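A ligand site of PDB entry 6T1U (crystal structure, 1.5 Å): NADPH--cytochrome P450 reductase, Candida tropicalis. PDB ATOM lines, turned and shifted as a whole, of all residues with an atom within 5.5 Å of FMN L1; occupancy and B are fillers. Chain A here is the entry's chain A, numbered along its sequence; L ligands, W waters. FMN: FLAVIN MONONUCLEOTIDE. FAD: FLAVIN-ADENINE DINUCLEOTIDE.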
ATOM      1  N   GLY A  64       3.868 -22.993  33.292  1.00  0.00           N
ATOM      2  CA  GLY A  64       5.188 -23.402  33.742  1.00  0.00           C
ATOM      3  C   GLY A  64       6.177 -22.567  32.928  1.00  0.00           C
ATOM      4  O   GLY A  64       6.391 -22.810  31.770  1.00  0.00           O
ATOM      5  N   SER A  65       6.784 -21.563  33.564  1.00  0.00           N
ATOM      6  CA  SER A  65       7.560 -20.574  32.823  1.00  0.00           C
ATOM      7  C   SER A  65       8.765 -20.154  33.652  1.00  0.00           C
ATOM      8  O   SER A  65       8.577 -19.925  34.868  1.00  0.00           O
ATOM      9  CB  SER A  65       6.695 -19.339  32.550  1.00  0.00           C
ATOM     10  OG  SER A  65       7.273 -18.430  31.649  1.00  0.00           O
ATOM     11  N   GLN A  66       9.926 -20.011  33.036  1.00  0.00           N
ATOM     12  CA  GLN A  66      11.124 -19.486  33.688  1.00  0.00           C
ATOM     13  C   GLN A  66      11.441 -18.059  33.247  1.00  0.00           C
ATOM     14  O   GLN A  66      11.837 -17.220  34.048  1.00  0.00           O
ATOM     15  CB  GLN A  66      12.310 -20.398  33.439  1.00  0.00           C
ATOM     16  CG  GLN A  66      13.466 -20.150  34.385  1.00  0.00           C
ATOM     17  CD  GLN A  66      13.188 -20.632  35.768  1.00  0.00           C
ATOM     18  OE1 GLN A  66      12.528 -21.661  35.977  1.00  0.00           O
ATOM     19  NE2 GLN A  66      13.740 -19.938  36.739  1.00  0.00           N
ATOM     20  N   THR A  67      11.297 -17.758  31.980  1.00  0.00           N
ATOM     21  CA  THR A  67      11.564 -16.434  31.420  1.00  0.00           C
ATOM     22  C   THR A  67      10.312 -15.776  30.833  1.00  0.00           C
ATOM     23  O   THR A  67      10.426 -14.855  30.037  1.00  0.00           O
ATOM     24  CB  THR A  67      12.747 -16.446  30.420  1.00  0.00           C
ATOM     25  OG1 THR A  67      12.563 -17.456  29.416  1.00  0.00           O
ATOM     26  CG2 THR A  67      14.073 -16.753  31.147  1.00  0.00           C
ATOM     27  N   GLY A  68       9.140 -16.261  31.228  1.00  0.00           N
ATOM     28  CA  GLY A  68       7.930 -15.535  30.979  1.00  0.00           C
ATOM     29  C   GLY A  68       7.145 -15.854  29.709  1.00  0.00           C
ATOM     30  O   GLY A  68       6.010 -15.376  29.599  1.00  0.00           O
ATOM     31  N   THR A  69       7.704 -16.621  28.786  1.00  0.00           N
ATOM     32  CA  THR A  69       7.007 -16.889  27.519  1.00  0.00           C
ATOM     33  C   THR A  69       5.735 -17.680  27.743  1.00  0.00           C
ATOM     34  O   THR A  69       4.679 -17.312  27.230  1.00  0.00           O
ATOM     35  CB  THR A  69       7.916 -17.638  26.555  1.00  0.00           C
ATOM     36  OG1 THR A  69       9.196 -16.989  26.553  1.00  0.00           O
ATOM     37  CG2 THR A  69       7.370 -17.670  25.145  1.00  0.00           C
ATOM     38  N   ALA A  70       5.848 -18.787  28.464  1.00  0.00           N
ATOM     39  CA  ALA A  70       4.672 -19.618  28.768  1.00  0.00           C
ATOM     40  C   ALA A  70       3.595 -18.835  29.520  1.00  0.00           C
ATOM     41  O   ALA A  70       2.414 -18.971  29.261  1.00  0.00           O
ATOM     42  CB  ALA A  70       5.027 -20.885  29.525  1.00  0.00           C
ATOM     43  N   GLU A  71       4.017 -17.949  30.412  1.00  0.00           N
ATOM     44  CA  GLU A  71       3.058 -17.058  31.092  1.00  0.00           C
ATOM     45  C   GLU A  71       2.330 -16.139  30.123  1.00  0.00           C
ATOM     46  O   GLU A  71       1.113 -15.970  30.171  1.00  0.00           O
ATOM     47  CB  GLU A  71       3.757 -16.232  32.188  1.00  0.00           C
ATOM     48  CG  GLU A  71       2.774 -15.375  32.977  1.00  0.00           C
ATOM     49  CD  GLU A  71       3.383 -14.601  34.129  1.00  0.00           C
ATOM     50  OE1 GLU A  71       2.635 -13.897  34.847  1.00  0.00           O
ATOM     51  OE2 GLU A  71       4.586 -14.678  34.340  1.00  0.00           O
ATOM     52  N   ALA A 116       6.812 -24.884  29.789  1.00  0.00           N
ATOM     53  CA  ALA A 116       8.164 -24.945  29.264  1.00  0.00           C
ATOM     54  C   ALA A 116       8.983 -26.057  29.891  1.00  0.00           C
ATOM     55  O   ALA A 116       8.765 -26.396  31.059  1.00  0.00           O
ATOM     56  CB  ALA A 116       8.888 -23.608  29.443  1.00  0.00           C
ATOM     57  N   THR A 117      10.007 -26.538  29.167  1.00  0.00           N
ATOM     58  CA  THR A 117      11.024 -27.448  29.722  1.00  0.00           C
ATOM     59  C   THR A 117      12.285 -26.615  30.006  1.00  0.00           C
ATOM     60  O   THR A 117      12.531 -25.633  29.315  1.00  0.00           O
ATOM     61  CB  THR A 117      11.308 -28.565  28.727  1.00  0.00           C
ATOM     62  OG1 THR A 117      10.080 -29.306  28.499  1.00  0.00           O
ATOM     63  CG2 THR A 117      12.351 -29.542  29.254  1.00  0.00           C
ATOM     64  N   TYR A 118      12.979 -26.911  31.122  1.00  0.00           N
ATOM     65  CA  TYR A 118      14.181 -26.133  31.512  1.00  0.00           C
ATOM     66  C   TYR A 118      15.298 -27.081  31.961  1.00  0.00           C
ATOM     67  O   TYR A 118      15.141 -28.275  31.936  1.00  0.00           O
ATOM     68  CB  TYR A 118      13.842 -25.072  32.568  1.00  0.00           C
ATOM     69  CG  TYR A 118      14.815 -23.886  32.709  1.00  0.00           C
ATOM     70  CD1 TYR A 118      15.101 -23.069  31.643  1.00  0.00           C
ATOM     71  CD2 TYR A 118      15.419 -23.592  33.951  1.00  0.00           C
ATOM     72  CE1 TYR A 118      15.968 -21.995  31.780  1.00  0.00           C
ATOM     73  CE2 TYR A 118      16.309 -22.541  34.092  1.00  0.00           C
ATOM     74  CZ  TYR A 118      16.570 -21.727  33.002  1.00  0.00           C
ATOM     75  OH  TYR A 118      17.449 -20.664  33.111  1.00  0.00           O
ATOM     76  N   GLY A 119      16.439 -26.475  32.316  1.00  0.00           N
ATOM     77  CA  GLY A 119      17.614 -27.237  32.745  1.00  0.00           C
ATOM     78  C   GLY A 119      17.809 -28.355  31.741  1.00  0.00           C
ATOM     79  O   GLY A 119      17.912 -28.091  30.533  1.00  0.00           O
ATOM     80  N   GLU A 120      17.764 -29.582  32.224  1.00  0.00           N
ATOM     81  CA  GLU A 120      18.035 -30.783  31.415  1.00  0.00           C
ATOM     82  C   GLU A 120      16.788 -31.641  31.449  1.00  0.00           C
ATOM     83  O   GLU A 120      16.719 -32.652  32.128  1.00  0.00           O
ATOM     84  CB  GLU A 120      19.270 -31.510  32.051  1.00  0.00           C
ATOM     85  CG  GLU A 120      20.072 -32.446  31.147  1.00  0.00           C
ATOM     86  CD  GLU A 120      20.768 -31.697  30.038  1.00  0.00           C
ATOM     87  OE1 GLU A 120      21.953 -31.309  30.257  1.00  0.00           O
ATOM     88  OE2 GLU A 120      20.124 -31.444  28.975  1.00  0.00           O
ATOM     89  N   GLY A 121      15.750 -31.244  30.700  1.00  0.00           N
ATOM     90  CA  GLY A 121      14.496 -31.963  30.734  1.00  0.00           C
ATOM     91  C   GLY A 121      13.695 -31.797  32.023  1.00  0.00           C
ATOM     92  O   GLY A 121      12.833 -32.593  32.318  1.00  0.00           O
ATOM     93  N   GLU A 122      13.962 -30.758  32.775  1.00  0.00           N
ATOM     94  CA  GLU A 122      13.376 -30.590  34.110  1.00  0.00           C
ATOM     95  C   GLU A 122      12.234 -29.563  34.031  1.00  0.00           C
ATOM     96  O   GLU A 122      12.134 -28.776  33.102  1.00  0.00           O
ATOM     97  CB  GLU A 122      14.439 -30.073  35.088  1.00  0.00           C
ATOM     98  CG  GLU A 122      15.667 -30.949  35.310  1.00  0.00           C
ATOM     99  CD  GLU A 122      16.826 -30.086  35.809  1.00  0.00           C
ATOM    100  OE1 GLU A 122      17.837 -29.840  35.094  1.00  0.00           O
ATOM    101  OE2 GLU A 122      16.704 -29.537  36.940  1.00  0.00           O
ATOM    102  N   THR A 124      10.281 -26.060  34.951  1.00  0.00           N
ATOM    103  CA  THR A 124      10.567 -24.690  35.410  1.00  0.00           C
ATOM    104  C   THR A 124      10.447 -24.660  36.933  1.00  0.00           C
ATOM    105  O   THR A 124       9.709 -25.438  37.521  1.00  0.00           O
ATOM    106  CB  THR A 124       9.615 -23.672  34.788  1.00  0.00           C
ATOM    107  OG1 THR A 124       8.263 -24.043  35.063  1.00  0.00           O
ATOM    108  CG2 THR A 124       9.793 -23.633  33.266  1.00  0.00           C
ATOM    109  N   LEU A 151       6.390 -25.828  25.568  1.00  0.00           N
ATOM    110  CA  LEU A 151       7.442 -24.950  25.014  1.00  0.00           C
ATOM    111  C   LEU A 151       8.788 -25.615  25.244  1.00  0.00           C
ATOM    112  O   LEU A 151       9.099 -26.039  26.380  1.00  0.00           O
ATOM    113  CB  LEU A 151       7.477 -23.576  25.652  1.00  0.00           C
ATOM    114  CG  LEU A 151       6.270 -22.663  25.469  1.00  0.00           C
ATOM    115  CD1 LEU A 151       5.012 -23.088  26.214  1.00  0.00           C
ATOM    116  CD2 LEU A 151       6.668 -21.235  25.883  1.00  0.00           C
ATOM    117  N   GLY A 152       9.583 -25.693  24.181  1.00  0.00           N
ATOM    118  CA  GLY A 152      10.917 -26.277  24.281  1.00  0.00           C
ATOM    119  C   GLY A 152      11.804 -25.811  23.159  1.00  0.00           C
ATOM    120  O   GLY A 152      11.583 -24.764  22.577  1.00  0.00           O
ATOM    121  N   ASN A 153      12.834 -26.584  22.871  1.00  0.00           N
ATOM    122  CA  ASN A 153      13.876 -26.173  21.959  1.00  0.00           C
ATOM    123  C   ASN A 153      14.600 -27.447  21.532  1.00  0.00           C
ATOM    124  O   ASN A 153      15.182 -28.111  22.350  1.00  0.00           O
ATOM    125  CB  ASN A 153      14.803 -25.167  22.675  1.00  0.00           C
ATOM    126  CG  ASN A 153      15.964 -24.753  21.832  1.00  0.00           C
ATOM    127  OD1 ASN A 153      16.468 -25.539  21.008  1.00  0.00           O
ATOM    128  ND2 ASN A 153      16.427 -23.519  22.030  1.00  0.00           N
ATOM    129  N   SER A 154      14.534 -27.777  20.231  1.00  0.00           N
ATOM    130  CA  SER A 154      15.009 -29.059  19.735  1.00  0.00           C
ATOM    131  C   SER A 154      16.529 -29.200  19.659  1.00  0.00           C
ATOM    132  O   SER A 154      17.042 -30.259  19.340  1.00  0.00           O
ATOM    133  CB  SER A 154      14.382 -29.346  18.360  1.00  0.00           C
ATOM    134  OG  SER A 154      14.768 -28.358  17.438  1.00  0.00           O
ATOM    135  N   TYR A 156      18.101 -29.035  22.437  1.00  0.00           N
ATOM    136  CA  TYR A 156      18.331 -29.724  23.717  1.00  0.00           C
ATOM    137  C   TYR A 156      17.909 -31.164  23.551  1.00  0.00           C
ATOM    138  O   TYR A 156      17.005 -31.468  22.792  1.00  0.00           O
ATOM    139  CB  TYR A 156      17.474 -29.073  24.813  1.00  0.00           C
ATOM    140  CG  TYR A 156      17.998 -27.718  25.191  1.00  0.00           C
ATOM    141  CD1 TYR A 156      17.685 -26.594  24.439  1.00  0.00           C
ATOM    142  CD2 TYR A 156      18.776 -27.552  26.328  1.00  0.00           C
ATOM    143  CE1 TYR A 156      18.186 -25.339  24.802  1.00  0.00           C
ATOM    144  CE2 TYR A 156      19.282 -26.315  26.679  1.00  0.00           C
ATOM    145  CZ  TYR A 156      18.981 -25.197  25.909  1.00  0.00           C
ATOM    146  OH  TYR A 156      19.438 -23.928  26.248  1.00  0.00           O
ATOM    147  N   PHE A 158      16.456 -33.386  25.647  1.00  0.00           N
ATOM    148  CA  PHE A 158      15.156 -33.776  26.216  1.00  0.00           C
ATOM    149  C   PHE A 158      14.077 -32.797  25.743  1.00  0.00           C
ATOM    150  O   PHE A 158      13.527 -31.987  26.479  1.00  0.00           O
ATOM    151  CB  PHE A 158      15.293 -33.874  27.749  1.00  0.00           C
ATOM    152  CG  PHE A 158      16.319 -34.894  28.182  1.00  0.00           C
ATOM    153  CD1 PHE A 158      16.065 -36.249  28.067  1.00  0.00           C
ATOM    154  CD2 PHE A 158      17.544 -34.495  28.632  1.00  0.00           C
ATOM    155  CE1 PHE A 158      17.024 -37.190  28.436  1.00  0.00           C
ATOM    156  CE2 PHE A 158      18.520 -35.423  29.007  1.00  0.00           C
ATOM    157  CZ  PHE A 158      18.251 -36.765  28.905  1.00  0.00           C
ATOM    158  N   PHE A 159      13.820 -32.819  24.452  1.00  0.00           N
ATOM    159  CA  PHE A 159      12.955 -31.836  23.802  1.00  0.00           C
ATOM    160  C   PHE A 159      11.566 -31.896  24.311  1.00  0.00           C
ATOM    161  O   PHE A 159      10.880 -32.921  24.201  1.00  0.00           O
ATOM    162  CB  PHE A 159      12.939 -32.119  22.305  1.00  0.00           C
ATOM    163  CG  PHE A 159      12.033 -31.194  21.499  1.00  0.00           C
ATOM    164  CD1 PHE A 159      12.161 -29.837  21.519  1.00  0.00           C
ATOM    165  CD2 PHE A 159      11.037 -31.716  20.659  1.00  0.00           C
ATOM    166  CE1 PHE A 159      11.355 -29.032  20.723  1.00  0.00           C
ATOM    167  CE2 PHE A 159      10.219 -30.920  19.902  1.00  0.00           C
ATOM    168  CZ  PHE A 159      10.365 -29.555  19.919  1.00  0.00           C
ATOM    169  N   ASN A 160      11.101 -30.768  24.862  1.00  0.00           N
ATOM    170  CA  ASN A 160       9.749 -30.659  25.381  1.00  0.00           C
ATOM    171  C   ASN A 160       9.402 -31.819  26.348  1.00  0.00           C
ATOM    172  O   ASN A 160       8.247 -32.230  26.413  1.00  0.00           O
ATOM    173  CB  ASN A 160       8.736 -30.566  24.255  1.00  0.00           C
ATOM    174  CG  ASN A 160       8.415 -29.125  23.887  1.00  0.00           C
ATOM    175  OD1 ASN A 160       7.895 -28.381  24.700  1.00  0.00           O
ATOM    176  ND2 ASN A 160       8.782 -28.712  22.669  1.00  0.00           N
ATOM    177  N   ALA A 161      10.394 -32.255  27.114  1.00  0.00           N
ATOM    178  CA  ALA A 161      10.176 -33.369  28.046  1.00  0.00           C
ATOM    179  C   ALA A 161       8.981 -33.093  28.939  1.00  0.00           C
ATOM    180  O   ALA A 161       8.187 -34.003  29.203  1.00  0.00           O
ATOM    181  CB  ALA A 161      11.405 -33.625  28.873  1.00  0.00           C
ATOM    182  N   ASP A 186      11.609 -23.296  20.134  1.00  0.00           N
ATOM    183  CA  ASP A 186      12.351 -22.062  20.199  1.00  0.00           C
ATOM    184  C   ASP A 186      13.727 -22.174  19.533  1.00  0.00           C
ATOM    185  O   ASP A 186      14.387 -21.161  19.276  1.00  0.00           O
ATOM    186  CB  ASP A 186      12.506 -21.672  21.684  1.00  0.00           C
ATOM    187  CG  ASP A 186      12.307 -20.218  21.949  1.00  0.00           C
ATOM    188  OD1 ASP A 186      11.966 -19.431  21.040  1.00  0.00           O
ATOM    189  OD2 ASP A 186      12.456 -19.882  23.151  1.00  0.00           O
ATOM    190  N   LEU A 191       8.372 -21.307  17.508  1.00  0.00           N
ATOM    191  CA  LEU A 191       7.571 -21.379  18.749  1.00  0.00           C
ATOM    192  C   LEU A 191       6.268 -20.618  18.654  1.00  0.00           C
ATOM    193  O   LEU A 191       5.205 -21.157  18.953  1.00  0.00           O
ATOM    194  CB  LEU A 191       8.406 -20.924  19.946  1.00  0.00           C
ATOM    195  CG  LEU A 191       7.635 -20.748  21.244  1.00  0.00           C
ATOM    196  CD1 LEU A 191       7.143 -22.070  21.709  1.00  0.00           C
ATOM    197  CD2 LEU A 191       8.554 -20.135  22.290  1.00  0.00           C
ATOM    198  N   VAL A 678      23.880 -24.470  29.353  1.00  0.00           N
ATOM    199  CA  VAL A 678      23.906 -24.031  27.932  1.00  0.00           C
ATOM    200  C   VAL A 678      22.636 -23.293  27.611  1.00  0.00           C
ATOM    201  O   VAL A 678      21.536 -23.672  28.069  1.00  0.00           O
ATOM    202  CB  VAL A 678      24.158 -25.196  26.950  1.00  0.00           C
ATOM    203  CG1 VAL A 678      25.537 -25.789  27.246  1.00  0.00           C
ATOM    204  CG2 VAL A 678      23.080 -26.258  26.992  1.00  0.00           C
ATOM    205  N   TRP A 679      22.783 -22.265  26.768  1.00  0.00           N
ATOM    206  CA  TRP A 679      21.670 -21.327  26.464  1.00  0.00           C
ATOM    207  C   TRP A 679      21.741 -20.929  25.002  1.00  0.00           C
ATOM    208  O   TRP A 679      22.754 -21.197  24.317  1.00  0.00           O
ATOM    209  CB  TRP A 679      21.725 -20.086  27.367  1.00  0.00           C
ATOM    210  CG  TRP A 679      22.969 -19.273  27.243  1.00  0.00           C
ATOM    211  CD1 TRP A 679      23.174 -18.261  26.369  1.00  0.00           C
ATOM    212  CD2 TRP A 679      24.168 -19.386  27.996  1.00  0.00           C
ATOM    213  NE1 TRP A 679      24.406 -17.722  26.541  1.00  0.00           N
ATOM    214  CE2 TRP A 679      25.062 -18.403  27.515  1.00  0.00           C
ATOM    215  CE3 TRP A 679      24.592 -20.223  29.023  1.00  0.00           C
ATOM    216  CZ2 TRP A 679      26.343 -18.256  28.034  1.00  0.00           C
ATOM    217  CZ3 TRP A 679      25.850 -20.051  29.537  1.00  0.00           C
ATOM    218  CH2 TRP A 679      26.696 -19.086  29.050  1.00  0.00           C
ATOM    219  OXT TRP A 679      20.805 -20.268  24.542  1.00  0.00           O
HETATM  220  N1  FMN L   1      13.753 -26.908  25.883  1.00  0.00           N
HETATM  221  C2  FMN L   1      13.632 -28.239  25.837  1.00  0.00           C
HETATM  222  O2  FMN L   1      12.836 -28.698  24.971  1.00  0.00           O
HETATM  223  N3  FMN L   1      14.324 -29.079  26.652  1.00  0.00           N
HETATM  224  C4  FMN L   1      15.210 -28.680  27.574  1.00  0.00           C
HETATM  225  O4  FMN L   1      15.837 -29.475  28.310  1.00  0.00           O
HETATM  226  C4A FMN L   1      15.435 -27.252  27.645  1.00  0.00           C
HETATM  227  N5  FMN L   1      16.305 -26.759  28.523  1.00  0.00           N
HETATM  228  C5A FMN L   1      16.584 -25.423  28.525  1.00  0.00           C
HETATM  229  C6  FMN L   1      17.555 -24.935  29.393  1.00  0.00           C
HETATM  230  C7  FMN L   1      17.807 -23.579  29.428  1.00  0.00           C
HETATM  231  C7M FMN L   1      18.829 -22.991  30.348  1.00  0.00           C
HETATM  232  C8  FMN L   1      17.048 -22.660  28.548  1.00  0.00           C
HETATM  233  C8M FMN L   1      17.259 -21.196  28.481  1.00  0.00           C
HETATM  234  C9  FMN L   1      16.103 -23.151  27.696  1.00  0.00           C
HETATM  235  C9A FMN L   1      15.812 -24.488  27.681  1.00  0.00           C
HETATM  236  N10 FMN L   1      14.813 -25.027  26.839  1.00  0.00           N
HETATM  237  C10 FMN L   1      14.650 -26.398  26.766  1.00  0.00           C
HETATM  238  C1' FMN L   1      14.033 -24.167  25.945  1.00  0.00           C
HETATM  239  C2' FMN L   1      12.923 -23.403  26.716  1.00  0.00           C
HETATM  240  O2' FMN L   1      11.895 -24.303  27.215  1.00  0.00           O
HETATM  241  C3' FMN L   1      12.278 -22.416  25.764  1.00  0.00           C
HETATM  242  O3' FMN L   1      13.193 -21.345  25.466  1.00  0.00           O
HETATM  243  C4' FMN L   1      10.960 -21.821  26.262  1.00  0.00           C
HETATM  244  O4' FMN L   1      10.302 -21.135  25.215  1.00  0.00           O
HETATM  245  C5' FMN L   1      11.074 -20.928  27.487  1.00  0.00           C
HETATM  246  O5' FMN L   1       9.778 -20.675  28.000  1.00  0.00           O
HETATM  247  P   FMN L   1       9.675 -19.672  29.277  1.00  0.00           P
HETATM  248  O1P FMN L   1       8.218 -19.671  29.592  1.00  0.00           O
HETATM  249  O2P FMN L   1      10.166 -18.277  28.804  1.00  0.00           O
HETATM  250  O3P FMN L   1      10.531 -20.216  30.379  1.00  0.00           O
HETATM  251  PA  FAD L   2      17.380  -9.503  24.581  1.00  0.00           P
HETATM  252  O1A FAD L   2      16.757  -8.173  24.743  1.00  0.00           O
HETATM  253  O2A FAD L   2      16.779 -10.644  25.301  1.00  0.00           O
HETATM  254  O5B FAD L   2      17.411  -9.744  23.007  1.00  0.00           O
HETATM  255  C5B FAD L   2      17.819 -11.028  22.505  1.00  0.00           C
HETATM  256  C4B FAD L   2      18.288 -10.891  21.074  1.00  0.00           C
HETATM  257  O4B FAD L   2      17.181 -10.441  20.242  1.00  0.00           O
HETATM  258  C3B FAD L   2      19.422  -9.893  20.843  1.00  0.00           C
HETATM  259  O3B FAD L   2      20.339 -10.369  19.850  1.00  0.00           O
HETATM  260  C2B FAD L   2      18.695  -8.679  20.319  1.00  0.00           C
HETATM  261  O2B FAD L   2      19.454  -7.728  19.575  1.00  0.00           O
HETATM  262  C1B FAD L   2      17.649  -9.399  19.437  1.00  0.00           C
HETATM  263  N9A FAD L   2      16.512  -8.566  19.110  1.00  0.00           N
HETATM  264  C8A FAD L   2      16.087  -7.412  19.709  1.00  0.00           C
HETATM  265  N7A FAD L   2      14.971  -6.951  19.147  1.00  0.00           N
HETATM  266  C5A FAD L   2      14.614  -7.855  18.192  1.00  0.00           C
HETATM  267  C6A FAD L   2      13.488  -8.003  17.295  1.00  0.00           C
HETATM  268  N6A FAD L   2      12.531  -7.081  17.262  1.00  0.00           N
HETATM  269  N1A FAD L   2      13.475  -9.087  16.481  1.00  0.00           N
HETATM  270  C2A FAD L   2      14.469 -10.015  16.534  1.00  0.00           C
HETATM  271  N3A FAD L   2      15.517  -9.955  17.379  1.00  0.00           N
HETATM  272  C4A FAD L   2      15.617  -8.896  18.182  1.00  0.00           C
HETATM  273  N1  FAD L   2      24.752 -14.524  28.352  1.00  0.00           N
HETATM  274  C2  FAD L   2      26.007 -14.083  28.537  1.00  0.00           C
HETATM  275  O2  FAD L   2      26.455 -13.229  27.780  1.00  0.00           O
HETATM  276  N3  FAD L   2      26.774 -14.579  29.544  1.00  0.00           N
HETATM  277  C4  FAD L   2      26.399 -15.553  30.355  1.00  0.00           C
HETATM  278  O4  FAD L   2      27.105 -15.988  31.285  1.00  0.00           O
HETATM  279  C4X FAD L   2      25.065 -16.078  30.210  1.00  0.00           C
HETATM  280  N5  FAD L   2      24.639 -17.091  31.003  1.00  0.00           N
HETATM  281  C5X FAD L   2      23.353 -17.537  30.899  1.00  0.00           C
HETATM  282  C6  FAD L   2      22.855 -18.552  31.731  1.00  0.00           C
HETATM  283  C7  FAD L   2      21.539 -18.995  31.576  1.00  0.00           C
HETATM  284  C7M FAD L   2      21.020 -20.102  32.505  1.00  0.00           C
HETATM  285  C8  FAD L   2      20.646 -18.414  30.563  1.00  0.00           C
HETATM  286  C8M FAD L   2      19.249 -18.879  30.400  1.00  0.00           C
HETATM  287  C9  FAD L   2      21.163 -17.445  29.725  1.00  0.00           C
HETATM  288  C9A FAD L   2      22.467 -16.979  29.866  1.00  0.00           C
HETATM  289  N10 FAD L   2      22.943 -15.946  29.020  1.00  0.00           N
HETATM  290  C10 FAD L   2      24.270 -15.484  29.155  1.00  0.00           C
HETATM  291  C1' FAD L   2      22.102 -15.282  28.012  1.00  0.00           C
HETATM  292  C2' FAD L   2      21.383 -14.053  28.651  1.00  0.00           C
HETATM  293  O2' FAD L   2      20.465 -14.468  29.636  1.00  0.00           O
HETATM  294  C3' FAD L   2      20.692 -13.203  27.645  1.00  0.00           C
HETATM  295  O3' FAD L   2      19.791 -14.051  26.911  1.00  0.00           O
HETATM  296  C4' FAD L   2      21.594 -12.409  26.718  1.00  0.00           C
HETATM  297  O4' FAD L   2      22.604 -11.727  27.467  1.00  0.00           O
HETATM  298  C5' FAD L   2      20.766 -11.444  25.885  1.00  0.00           C
HETATM  299  O5' FAD L   2      20.043 -10.572  26.764  1.00  0.00           O
HETATM  300  P   FAD L   2      19.654  -9.097  26.323  1.00  0.00           P
HETATM  301  O1P FAD L   2      18.660  -8.560  27.273  1.00  0.00           O
HETATM  302  O2P FAD L   2      20.842  -8.282  25.984  1.00  0.00           O
HETATM  303  O3P FAD L   2      18.957  -9.376  24.877  1.00  0.00           O
HETATM  304  O   HOH W   1      15.552 -21.603  23.902  1.00  0.00           O
HETATM  305  O   HOH W   2      14.484 -19.706  27.260  1.00  0.00           O
HETATM  306  O   HOH W   3      17.617 -31.359  27.504  1.00  0.00           O
HETATM  307  O   HOH W   4      10.961 -18.359  24.950  1.00  0.00           O
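Water W3 lies within hydrogen-bond range of O4 of FMN L1 (2.7 Å), OE2 of Glu 120 (2.9 Å) and N of Phe 158 (3.0 Å). Water W1 bridges ND2 of Asn 153 and O3' of FMN L1. Water W4 lies within hydrogen-bond range of OG1 of Thr 69 (2.7 Å), OD2 of Asp 186 (2.8 Å) and O4' of FMN L1 (2.9 Å).
The backbone NH (N) of Thr 117 is in hydrogen-bond range of the backbone carbonyl oxygen (O) of Leu 151, at 3.0 Å. The side-chain hydroxyl (OG1) of Thr 117 lies within hydrogen-bond range of the backbone NH (N) of Ala 161 (3.3 Å). OG of Ser 65 sits at hydrogen-bond distance from N of Thr 69 (3.4 Å). The side-chain hydroxyl (OG) of Ser 65 is in hydrogen-bond range of the backbone NH (N) of Gly 68 (2.9 Å). N of Ser 65 sits at hydrogen-bond distance from OG1 of Thr 124, at 3.3 Å. OD1 of Asn 160 lies within hydrogen-bond range of N of Gly 152, at 3.2 Å. The backbone NH (N) of Ala 116 sits at hydrogen-bond distance from the backbone carbonyl oxygen (O) of Gly 64 (2.9 Å). OE1 of Glu 122 is in hydrogen-bond range of N of Glu 120 (2.9 Å).
N5 of FMN L1 lies close to O of Gly 119, 2.9 Å away. Ala 116 touches FMN L1 (CB to O5', 3.4 Å). Tyr 118 touches FMN L1 (CE1 to C7M, 3.4 Å). Glu 120 touches FMN L1 (C to O4, 3.9 Å). Gly 152 touches FMN L1 (CA to O2, 3.2 Å). Tyr 156 touches FMN L1 (CE2 to C5A, 3.4 Å). CA of Phe 159 touches O2 of FMN L1 (3.4 Å). Leu 191 touches FMN L1 (CD2 to O4', 3.6 Å). O of Val 678 touches C7M of FMN L1, 3.6 Å away.
O of Thr 117 is in hydrogen-bond range of O2' of FMN L1 (2.6 Å). An oxygen (O1P) of FMN L1 lies within hydrogen-bond range of the side-chain hydroxyl of Ser 65, at 2.6 Å. The backbone NH (N) of Thr 67 is in hydrogen-bond range of an oxygen (O3P) of FMN L1, at 3.0 Å. O2P of FMN L1 sits at hydrogen-bond distance from OG1 of Thr 67 (2.6 Å). An oxygen (O2) of FMN L1 is in hydrogen-bond range of the backbone NH (N) of Asn 160, 2.7 Å away. O3P of FMN L1 is in hydrogen-bond range of N of Gln 66 (2.7 Å). The backbone NH of Thr 69 sits at hydrogen-bond distance from an oxygen (O2P) of FMN L1 (3.0 Å). OG1 of Thr 69 lies within hydrogen-bond range of O2P of FMN L1. N of Ala 70 lies within hydrogen-bond range of O1P of FMN L1 (2.8 Å). An oxygen (O3') of FMN L1 sits at hydrogen-bond distance from the side-chain carboxylate (OD2) of Asp 186 (2.8 Å). N of Gly 121 lies within hydrogen-bond range of O4 of FMN L1 (3.0 Å). An oxygen (O2) of FMN L1 sits at hydrogen-bond distance from the backbone NH (N) of Asn 153 (3.0 Å). A nitrogen (N3) of FMN L1 lies within hydrogen-bond range of the backbone carbonyl oxygen of Phe 158 (3.0 Å). N of Gly 68 is in hydrogen-bond range of O2P of FMN L1 (3.3 Å). O2' of FMN L1 lies within hydrogen-bond range of O of Leu 151 (3.4 Å).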
